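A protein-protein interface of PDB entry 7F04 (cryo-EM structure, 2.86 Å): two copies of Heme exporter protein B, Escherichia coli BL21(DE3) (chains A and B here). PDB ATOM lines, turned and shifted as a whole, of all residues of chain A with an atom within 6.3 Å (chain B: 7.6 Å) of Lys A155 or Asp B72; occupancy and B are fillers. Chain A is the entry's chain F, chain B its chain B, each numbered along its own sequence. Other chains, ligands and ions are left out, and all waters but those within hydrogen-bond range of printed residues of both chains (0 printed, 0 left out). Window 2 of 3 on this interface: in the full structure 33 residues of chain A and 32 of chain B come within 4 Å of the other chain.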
ATOM      1  N   ARG A  71      11.276  -1.990 -26.982  1.00  0.00           N
ATOM      2  CA  ARG A  71      11.614  -0.801 -27.755  1.00  0.00           C
ATOM      3  C   ARG A  71      12.246  -1.160 -29.093  1.00  0.00           C
ATOM      4  O   ARG A  71      11.775  -0.721 -30.147  1.00  0.00           O
ATOM      5  CB  ARG A  71      12.536   0.079 -26.912  1.00  0.00           C
ATOM      6  CG  ARG A  71      12.929   1.442 -27.445  1.00  0.00           C
ATOM      7  CD  ARG A  71      14.149   1.352 -28.333  1.00  0.00           C
ATOM      8  NE  ARG A  71      15.248   0.721 -27.611  1.00  0.00           N
ATOM      9  CZ  ARG A  71      16.052   1.342 -26.761  1.00  0.00           C
ATOM     10  NH1 ARG A  71      15.863   2.608 -26.432  1.00  0.00           N
ATOM     11  NH2 ARG A  71      17.054   0.668 -26.206  1.00  0.00           N
ATOM     12  N   GLN A  75      10.576  -1.247 -34.353  1.00  0.00           N
ATOM     13  CA  GLN A  75      11.266  -0.779 -35.551  1.00  0.00           C
ATOM     14  C   GLN A  75      11.522  -1.922 -36.522  1.00  0.00           C
ATOM     15  O   GLN A  75      11.389  -1.749 -37.739  1.00  0.00           O
ATOM     16  CB  GLN A  75      12.582  -0.089 -35.193  1.00  0.00           C
ATOM     17  CG  GLN A  75      12.433   1.214 -34.435  1.00  0.00           C
ATOM     18  CD  GLN A  75      12.457   1.014 -32.941  1.00  0.00           C
ATOM     19  OE1 GLN A  75      12.939  -0.006 -32.454  1.00  0.00           O
ATOM     20  NE2 GLN A  75      11.931   1.983 -32.200  1.00  0.00           N
ATOM     21  N   THR A 151       3.189   1.910 -24.451  1.00  0.00           N
ATOM     22  CA  THR A 151       3.954   3.071 -24.881  1.00  0.00           C
ATOM     23  C   THR A 151       5.023   2.742 -25.918  1.00  0.00           C
ATOM     24  O   THR A 151       5.815   3.621 -26.269  1.00  0.00           O
ATOM     25  CB  THR A 151       4.604   3.751 -23.673  1.00  0.00           C
ATOM     26  OG1 THR A 151       5.488   2.830 -23.023  1.00  0.00           O
ATOM     27  CG2 THR A 151       3.545   4.205 -22.685  1.00  0.00           C
ATOM     28  N   VAL A 152       5.074   1.502 -26.411  1.00  0.00           N
ATOM     29  CA  VAL A 152       6.119   1.133 -27.361  1.00  0.00           C
ATOM     30  C   VAL A 152       5.932   1.867 -28.685  1.00  0.00           C
ATOM     31  O   VAL A 152       6.909   2.255 -29.336  1.00  0.00           O
ATOM     32  CB  VAL A 152       6.165  -0.396 -27.550  1.00  0.00           C
ATOM     33  CG1 VAL A 152       4.882  -0.916 -28.179  1.00  0.00           C
ATOM     34  CG2 VAL A 152       7.367  -0.790 -28.385  1.00  0.00           C
ATOM     35  N   GLY A 153       4.681   2.074 -29.103  1.00  0.00           N
ATOM     36  CA  GLY A 153       4.434   2.792 -30.348  1.00  0.00           C
ATOM     37  C   GLY A 153       4.834   4.255 -30.239  1.00  0.00           C
ATOM     38  O   GLY A 153       5.248   4.861 -31.233  1.00  0.00           O
ATOM     39  N   LEU A 154       4.715   4.833 -29.045  1.00  0.00           N
ATOM     40  CA  LEU A 154       5.042   6.240 -28.856  1.00  0.00           C
ATOM     41  C   LEU A 154       6.546   6.466 -28.813  1.00  0.00           C
ATOM     42  O   LEU A 154       7.026   7.507 -29.275  1.00  0.00           O
ATOM     43  CB  LEU A 154       4.385   6.741 -27.573  1.00  0.00           C
ATOM     44  CG  LEU A 154       2.987   6.154 -27.371  1.00  0.00           C
ATOM     45  CD1 LEU A 154       2.429   6.529 -26.016  1.00  0.00           C
ATOM     46  CD2 LEU A 154       2.052   6.595 -28.482  1.00  0.00           C
ATOM     47  N   LYS A 155       7.294   5.505 -28.274  1.00  0.00           N
ATOM     48  CA  LYS A 155       8.749   5.586 -28.139  1.00  0.00           C
ATOM     49  C   LYS A 155       9.157   6.904 -27.480  1.00  0.00           C
ATOM     50  O   LYS A 155      10.034   7.633 -27.949  1.00  0.00           O
ATOM     51  CB  LYS A 155       9.440   5.396 -29.492  1.00  0.00           C
ATOM     52  CG  LYS A 155      10.917   5.041 -29.400  1.00  0.00           C
ATOM     53  CD  LYS A 155      11.559   5.001 -30.774  1.00  0.00           C
ATOM     54  CE  LYS A 155      11.776   6.404 -31.317  1.00  0.00           C
ATOM     55  NZ  LYS A 155      12.591   6.401 -32.562  1.00  0.00           N
ATOM     56  N   ARG A 156       8.474   7.209 -26.380  1.00  0.00           N
ATOM     57  CA  ARG A 156       8.782   8.393 -25.588  1.00  0.00           C
ATOM     58  C   ARG A 156      10.194   8.308 -25.016  1.00  0.00           C
ATOM     59  O   ARG A 156      10.967   9.267 -25.107  1.00  0.00           O
ATOM     60  CB  ARG A 156       7.751   8.549 -24.465  1.00  0.00           C
ATOM     61  CG  ARG A 156       6.347   8.821 -24.964  1.00  0.00           C
ATOM     62  CD  ARG A 156       6.217  10.236 -25.484  1.00  0.00           C
ATOM     63  NE  ARG A 156       4.881  10.501 -26.001  1.00  0.00           N
ATOM     64  CZ  ARG A 156       4.499  11.658 -26.522  1.00  0.00           C
ATOM     65  NH1 ARG A 156       5.315  12.697 -26.566  1.00  0.00           N
ATOM     66  NH2 ARG A 156       3.268  11.776 -27.007  1.00  0.00           N
ATOM     67  N   GLY A 157      10.544   7.161 -24.444  1.00  0.00           N
ATOM     68  CA  GLY A 157      11.830   7.028 -23.782  1.00  0.00           C
ATOM     69  C   GLY A 157      12.017   8.046 -22.681  1.00  0.00           C
ATOM     70  O   GLY A 157      13.112   8.603 -22.532  1.00  0.00           O
ATOM     71  N   GLY A 158      10.968   8.310 -21.909  1.00  0.00           N
ATOM     72  CA  GLY A 158      11.018   9.376 -20.931  1.00  0.00           C
ATOM     73  C   GLY A 158      10.043   9.228 -19.783  1.00  0.00           C
ATOM     74  O   GLY A 158       9.847   8.131 -19.251  1.00  0.00           O
ATOM     75  N   VAL B  13       9.375  17.924 -30.881  1.00  0.00           N
ATOM     76  CA  VAL B  13       9.373  16.466 -30.825  1.00  0.00           C
ATOM     77  C   VAL B  13       9.135  15.934 -29.422  1.00  0.00           C
ATOM     78  O   VAL B  13       8.815  14.752 -29.265  1.00  0.00           O
ATOM     79  CB  VAL B  13      10.689  15.880 -31.377  1.00  0.00           C
ATOM     80  CG1 VAL B  13      10.942  16.376 -32.788  1.00  0.00           C
ATOM     81  CG2 VAL B  13      11.849  16.220 -30.466  1.00  0.00           C
ATOM     82  N   ARG B  16       3.853  17.251 -27.996  1.00  0.00           N
ATOM     83  CA  ARG B  16       3.046  17.203 -29.203  1.00  0.00           C
ATOM     84  C   ARG B  16       1.637  17.738 -29.001  1.00  0.00           C
ATOM     85  O   ARG B  16       0.940  17.994 -29.989  1.00  0.00           O
ATOM     86  CB  ARG B  16       2.992  15.764 -29.729  1.00  0.00           C
ATOM     87  CG  ARG B  16       4.346  15.299 -30.233  1.00  0.00           C
ATOM     88  CD  ARG B  16       4.335  13.881 -30.756  1.00  0.00           C
ATOM     89  NE  ARG B  16       5.656  13.509 -31.245  1.00  0.00           N
ATOM     90  CZ  ARG B  16       6.598  12.938 -30.508  1.00  0.00           C
ATOM     91  NH1 ARG B  16       6.393  12.636 -29.237  1.00  0.00           N
ATOM     92  NH2 ARG B  16       7.779  12.666 -31.058  1.00  0.00           N
ATOM     93  N   ALA B  65      15.692  11.480 -20.235  1.00  0.00           N
ATOM     94  CA  ALA B  65      15.655  12.344 -21.406  1.00  0.00           C
ATOM     95  C   ALA B  65      16.944  12.324 -22.217  1.00  0.00           C
ATOM     96  O   ALA B  65      16.932  12.768 -23.370  1.00  0.00           O
ATOM     97  CB  ALA B  65      15.337  13.777 -20.991  1.00  0.00           C
ATOM     98  N   LEU B  66      18.051  11.838 -21.654  1.00  0.00           N
ATOM     99  CA  LEU B  66      19.296  11.790 -22.413  1.00  0.00           C
ATOM    100  C   LEU B  66      19.264  10.711 -23.484  1.00  0.00           C
ATOM    101  O   LEU B  66      19.881  10.873 -24.542  1.00  0.00           O
ATOM    102  CB  LEU B  66      20.479  11.566 -21.473  1.00  0.00           C
ATOM    103  CG  LEU B  66      21.174  12.825 -20.954  1.00  0.00           C
ATOM    104  CD1 LEU B  66      22.275  12.460 -19.977  1.00  0.00           C
ATOM    105  CD2 LEU B  66      21.725  13.649 -22.101  1.00  0.00           C
ATOM    106  N   GLU B  67      18.569   9.602 -23.228  1.00  0.00           N
ATOM    107  CA  GLU B  67      18.446   8.562 -24.244  1.00  0.00           C
ATOM    108  C   GLU B  67      17.671   9.068 -25.453  1.00  0.00           C
ATOM    109  O   GLU B  67      18.019   8.761 -26.597  1.00  0.00           O
ATOM    110  CB  GLU B  67      17.773   7.326 -23.648  1.00  0.00           C
ATOM    111  CG  GLU B  67      18.255   6.964 -22.252  1.00  0.00           C
ATOM    112  CD  GLU B  67      19.760   6.801 -22.168  1.00  0.00           C
ATOM    113  OE1 GLU B  67      20.363   6.293 -23.137  1.00  0.00           O
ATOM    114  OE2 GLU B  67      20.341   7.181 -21.130  1.00  0.00           O
ATOM    115  N   ARG B  68      16.620   9.852 -25.215  1.00  0.00           N
ATOM    116  CA  ARG B  68      15.846  10.432 -26.305  1.00  0.00           C
ATOM    117  C   ARG B  68      16.647  11.461 -27.095  1.00  0.00           C
ATOM    118  O   ARG B  68      16.287  11.770 -28.236  1.00  0.00           O
ATOM    119  CB  ARG B  68      14.572  11.064 -25.736  1.00  0.00           C
ATOM    120  CG  ARG B  68      13.583  11.579 -26.765  1.00  0.00           C
ATOM    121  CD  ARG B  68      12.859  12.809 -26.249  1.00  0.00           C
ATOM    122  NE  ARG B  68      11.835  12.479 -25.265  1.00  0.00           N
ATOM    123  CZ  ARG B  68      10.580  12.172 -25.563  1.00  0.00           C
ATOM    124  NH1 ARG B  68      10.155  12.135 -26.816  1.00  0.00           N
ATOM    125  NH2 ARG B  68       9.729  11.892 -24.580  1.00  0.00           N
ATOM    126  N   LEU B  69      17.731  11.986 -26.521  1.00  0.00           N
ATOM    127  CA  LEU B  69      18.451  13.093 -27.144  1.00  0.00           C
ATOM    128  C   LEU B  69      19.117  12.673 -28.450  1.00  0.00           C
ATOM    129  O   LEU B  69      18.942  13.329 -29.484  1.00  0.00           O
ATOM    130  CB  LEU B  69      19.487  13.650 -26.168  1.00  0.00           C
ATOM    131  CG  LEU B  69      20.141  14.982 -26.527  1.00  0.00           C
ATOM    132  CD1 LEU B  69      19.291  16.139 -26.038  1.00  0.00           C
ATOM    133  CD2 LEU B  69      21.530  15.058 -25.927  1.00  0.00           C
ATOM    134  N   PHE B  70      19.874  11.583 -28.429  1.00  0.00           N
ATOM    135  CA  PHE B  70      20.670  11.187 -29.587  1.00  0.00           C
ATOM    136  C   PHE B  70      20.256   9.854 -30.185  1.00  0.00           C
ATOM    137  O   PHE B  70      20.359   9.676 -31.399  1.00  0.00           O
ATOM    138  CB  PHE B  70      22.157  11.122 -29.212  1.00  0.00           C
ATOM    139  CG  PHE B  70      22.818  12.465 -29.117  1.00  0.00           C
ATOM    140  CD1 PHE B  70      22.636  13.412 -30.109  1.00  0.00           C
ATOM    141  CD2 PHE B  70      23.617  12.781 -28.035  1.00  0.00           C
ATOM    142  CE1 PHE B  70      23.241  14.648 -30.022  1.00  0.00           C
ATOM    143  CE2 PHE B  70      24.222  14.013 -27.945  1.00  0.00           C
ATOM    144  CZ  PHE B  70      24.035  14.948 -28.938  1.00  0.00           C
ATOM    145  N   ARG B  71      19.784   8.915 -29.364  1.00  0.00           N
ATOM    146  CA  ARG B  71      19.502   7.568 -29.852  1.00  0.00           C
ATOM    147  C   ARG B  71      18.447   7.564 -30.946  1.00  0.00           C
ATOM    148  O   ARG B  71      18.607   6.870 -31.954  1.00  0.00           O
ATOM    149  CB  ARG B  71      19.054   6.681 -28.694  1.00  0.00           C
ATOM    150  CG  ARG B  71      18.655   5.274 -29.093  1.00  0.00           C
ATOM    151  CD  ARG B  71      18.443   4.413 -27.854  1.00  0.00           C
ATOM    152  NE  ARG B  71      17.509   4.972 -26.875  1.00  0.00           N
ATOM    153  CZ  ARG B  71      16.320   5.508 -27.134  1.00  0.00           C
ATOM    154  NH1 ARG B  71      15.793   5.495 -28.348  1.00  0.00           N
ATOM    155  NH2 ARG B  71      15.622   6.042 -26.136  1.00  0.00           N
ATOM    156  N   ASP B  72      17.370   8.331 -30.773  1.00  0.00           N
ATOM    157  CA  ASP B  72      16.298   8.347 -31.759  1.00  0.00           C
ATOM    158  C   ASP B  72      16.727   8.977 -33.076  1.00  0.00           C
ATOM    159  O   ASP B  72      16.041   8.796 -34.087  1.00  0.00           O
ATOM    160  CB  ASP B  72      15.085   9.089 -31.201  1.00  0.00           C
ATOM    161  CG  ASP B  72      14.467   8.381 -30.012  1.00  0.00           C
ATOM    162  OD1 ASP B  72      14.590   7.143 -29.927  1.00  0.00           O
ATOM    163  OD2 ASP B  72      13.858   9.065 -29.162  1.00  0.00           O
ATOM    164  N   ASP B  73      17.839   9.711 -33.089  1.00  0.00           N
ATOM    165  CA  ASP B  73      18.278  10.391 -34.300  1.00  0.00           C
ATOM    166  C   ASP B  73      19.136   9.501 -35.190  1.00  0.00           C
ATOM    167  O   ASP B  73      19.202   9.731 -36.402  1.00  0.00           O
ATOM    168  CB  ASP B  73      19.044  11.659 -33.934  1.00  0.00           C
ATOM    169  CG  ASP B  73      18.155  12.719 -33.325  1.00  0.00           C
ATOM    170  OD1 ASP B  73      16.956  12.748 -33.662  1.00  0.00           O
ATOM    171  OD2 ASP B  73      18.653  13.522 -32.510  1.00  0.00           O
ATOM    172  N   LEU B  74      19.804   8.497 -34.621  1.00  0.00           N
ATOM    173  CA  LEU B  74      20.620   7.601 -35.436  1.00  0.00           C
ATOM    174  C   LEU B  74      19.772   6.804 -36.418  1.00  0.00           C
ATOM    175  O   LEU B  74      20.191   6.568 -37.557  1.00  0.00           O
ATOM    176  CB  LEU B  74      21.436   6.656 -34.555  1.00  0.00           C
ATOM    177  CG  LEU B  74      22.766   7.141 -33.975  1.00  0.00           C
ATOM    178  CD1 LEU B  74      23.744   7.419 -35.102  1.00  0.00           C
ATOM    179  CD2 LEU B  74      22.612   8.364 -33.096  1.00  0.00           C
ATOM    180  N   GLN B  75      18.584   6.366 -35.995  1.00  0.00           N
ATOM    181  CA  GLN B  75      17.742   5.586 -36.896  1.00  0.00           C
ATOM    182  C   GLN B  75      17.323   6.402 -38.112  1.00  0.00           C
ATOM    183  O   GLN B  75      17.275   5.874 -39.228  1.00  0.00           O
ATOM    184  CB  GLN B  75      16.516   5.044 -36.162  1.00  0.00           C
ATOM    185  CG  GLN B  75      16.827   3.935 -35.171  1.00  0.00           C
ATOM    186  CD  GLN B  75      17.160   4.462 -33.798  1.00  0.00           C
ATOM    187  OE1 GLN B  75      16.830   5.597 -33.467  1.00  0.00           O
ATOM    188  NE2 GLN B  75      17.818   3.640 -32.989  1.00  0.00           N
ATOM    189  N   ASP B  76      17.002   7.682 -37.926  1.00  0.00           N
ATOM    190  CA  ASP B  76      16.591   8.507 -39.056  1.00  0.00           C
ATOM    191  C   ASP B  76      17.544   9.662 -39.338  1.00  0.00           C
ATOM    192  O   ASP B  76      18.149   9.696 -40.414  1.00  0.00           O
ATOM    193  CB  ASP B  76      15.162   9.020 -38.822  1.00  0.00           C
ATOM    194  CG  ASP B  76      14.988   9.688 -37.471  1.00  0.00           C
ATOM    195  OD1 ASP B  76      15.666  10.702 -37.208  1.00  0.00           O
ATOM    196  OD2 ASP B  76      14.168   9.200 -36.668  1.00  0.00           O
ATOM    197  N   GLY B  77      17.735  10.589 -38.401  1.00  0.00           N
ATOM    198  CA  GLY B  77      18.307  11.874 -38.761  1.00  0.00           C
ATOM    199  C   GLY B  77      19.323  12.493 -37.823  1.00  0.00           C
ATOM    200  O   GLY B  77      19.293  13.707 -37.608  1.00  0.00           O
ATOM    201  N   SER B  78      20.214  11.685 -37.242  1.00  0.00           N
ATOM    202  CA  SER B  78      21.369  12.256 -36.554  1.00  0.00           C
ATOM    203  C   SER B  78      22.240  13.021 -37.536  1.00  0.00           C
ATOM    204  O   SER B  78      22.762  14.094 -37.216  1.00  0.00           O
ATOM    205  CB  SER B  78      22.176  11.162 -35.857  1.00  0.00           C
ATOM    206  OG  SER B  78      23.171  11.719 -35.015  1.00  0.00           O
ATOM    207  N   VAL B 152      24.944   5.428 -27.236  1.00  0.00           N
ATOM    208  CA  VAL B 152      23.755   5.142 -28.040  1.00  0.00           C
ATOM    209  C   VAL B 152      24.055   5.004 -29.520  1.00  0.00           C
ATOM    210  O   VAL B 152      23.137   4.715 -30.299  1.00  0.00           O
ATOM    211  CB  VAL B 152      22.672   6.228 -27.875  1.00  0.00           C
ATOM    212  CG1 VAL B 152      22.377   6.469 -26.402  1.00  0.00           C
ATOM    213  CG2 VAL B 152      23.083   7.510 -28.580  1.00  0.00           C
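NH2 of Arg B68 is in hydrogen-bond range of O of Arg A156.
NZ of Lys A155 is in salt-bridge range of OD1 of Asp B72 (3.4 Å).
NE of Arg B71 sits close to NH1 of Arg A71, at 2.9 Å.
NH1 of Arg B16 sits close to NH1 of Arg A156, at 2.9 Å.
The backbone carbonyl oxygen (O) of Val B13 sits at hydrogen-bond distance from the guanidinium group (NH2) of Arg B16 (2.9 Å).
NH1 of Arg B71 is in salt-bridge range of OD1 of Asp B72 (2.6 Å).
The side-chain amide oxygen (OE1) of Gln B75 sits close to the backbone carbonyl oxygen (O) of Arg B71 (2.7 Å).
O of Asp B72 sits close to OE1 of Gln B75 (3.4 Å).
O of Arg A71 lies close to OE1 of Gln A75, at 2.7 Å.
Printed residues of chain B within 4 Å of Lys A155: Asp B72 (3.2 Å).
Printed residues of chain A within 4 Å of Asp B72: Lys A155 (3.2 Å).
Of the printed residues of chain A, Arg B16 touches Arg A156.
Of the printed residues of chain B, Arg A71 touches Arg B71.
Glu B67 touches none of the printed residues of chain A.
Val A152 touches none of the printed residues of chain B.
The nearest residue of chain B that does not touch Lys A155 is Gln B75 (4.4 Å).
The nearest residue of chain A that does not touch Asp B72 is Arg A156 (5.0 Å).
Printed residues of chain B that touch a printed residue of chain A: Arg B16, Arg B68, Arg B71 and Asp B72.
Along chain A the printed residues that touch a printed residue of chain B span positions 71 to 156.
Arg B71 touches its own counterpart, Arg A71.
Positions printed for both chains: 71, 75 and 152.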
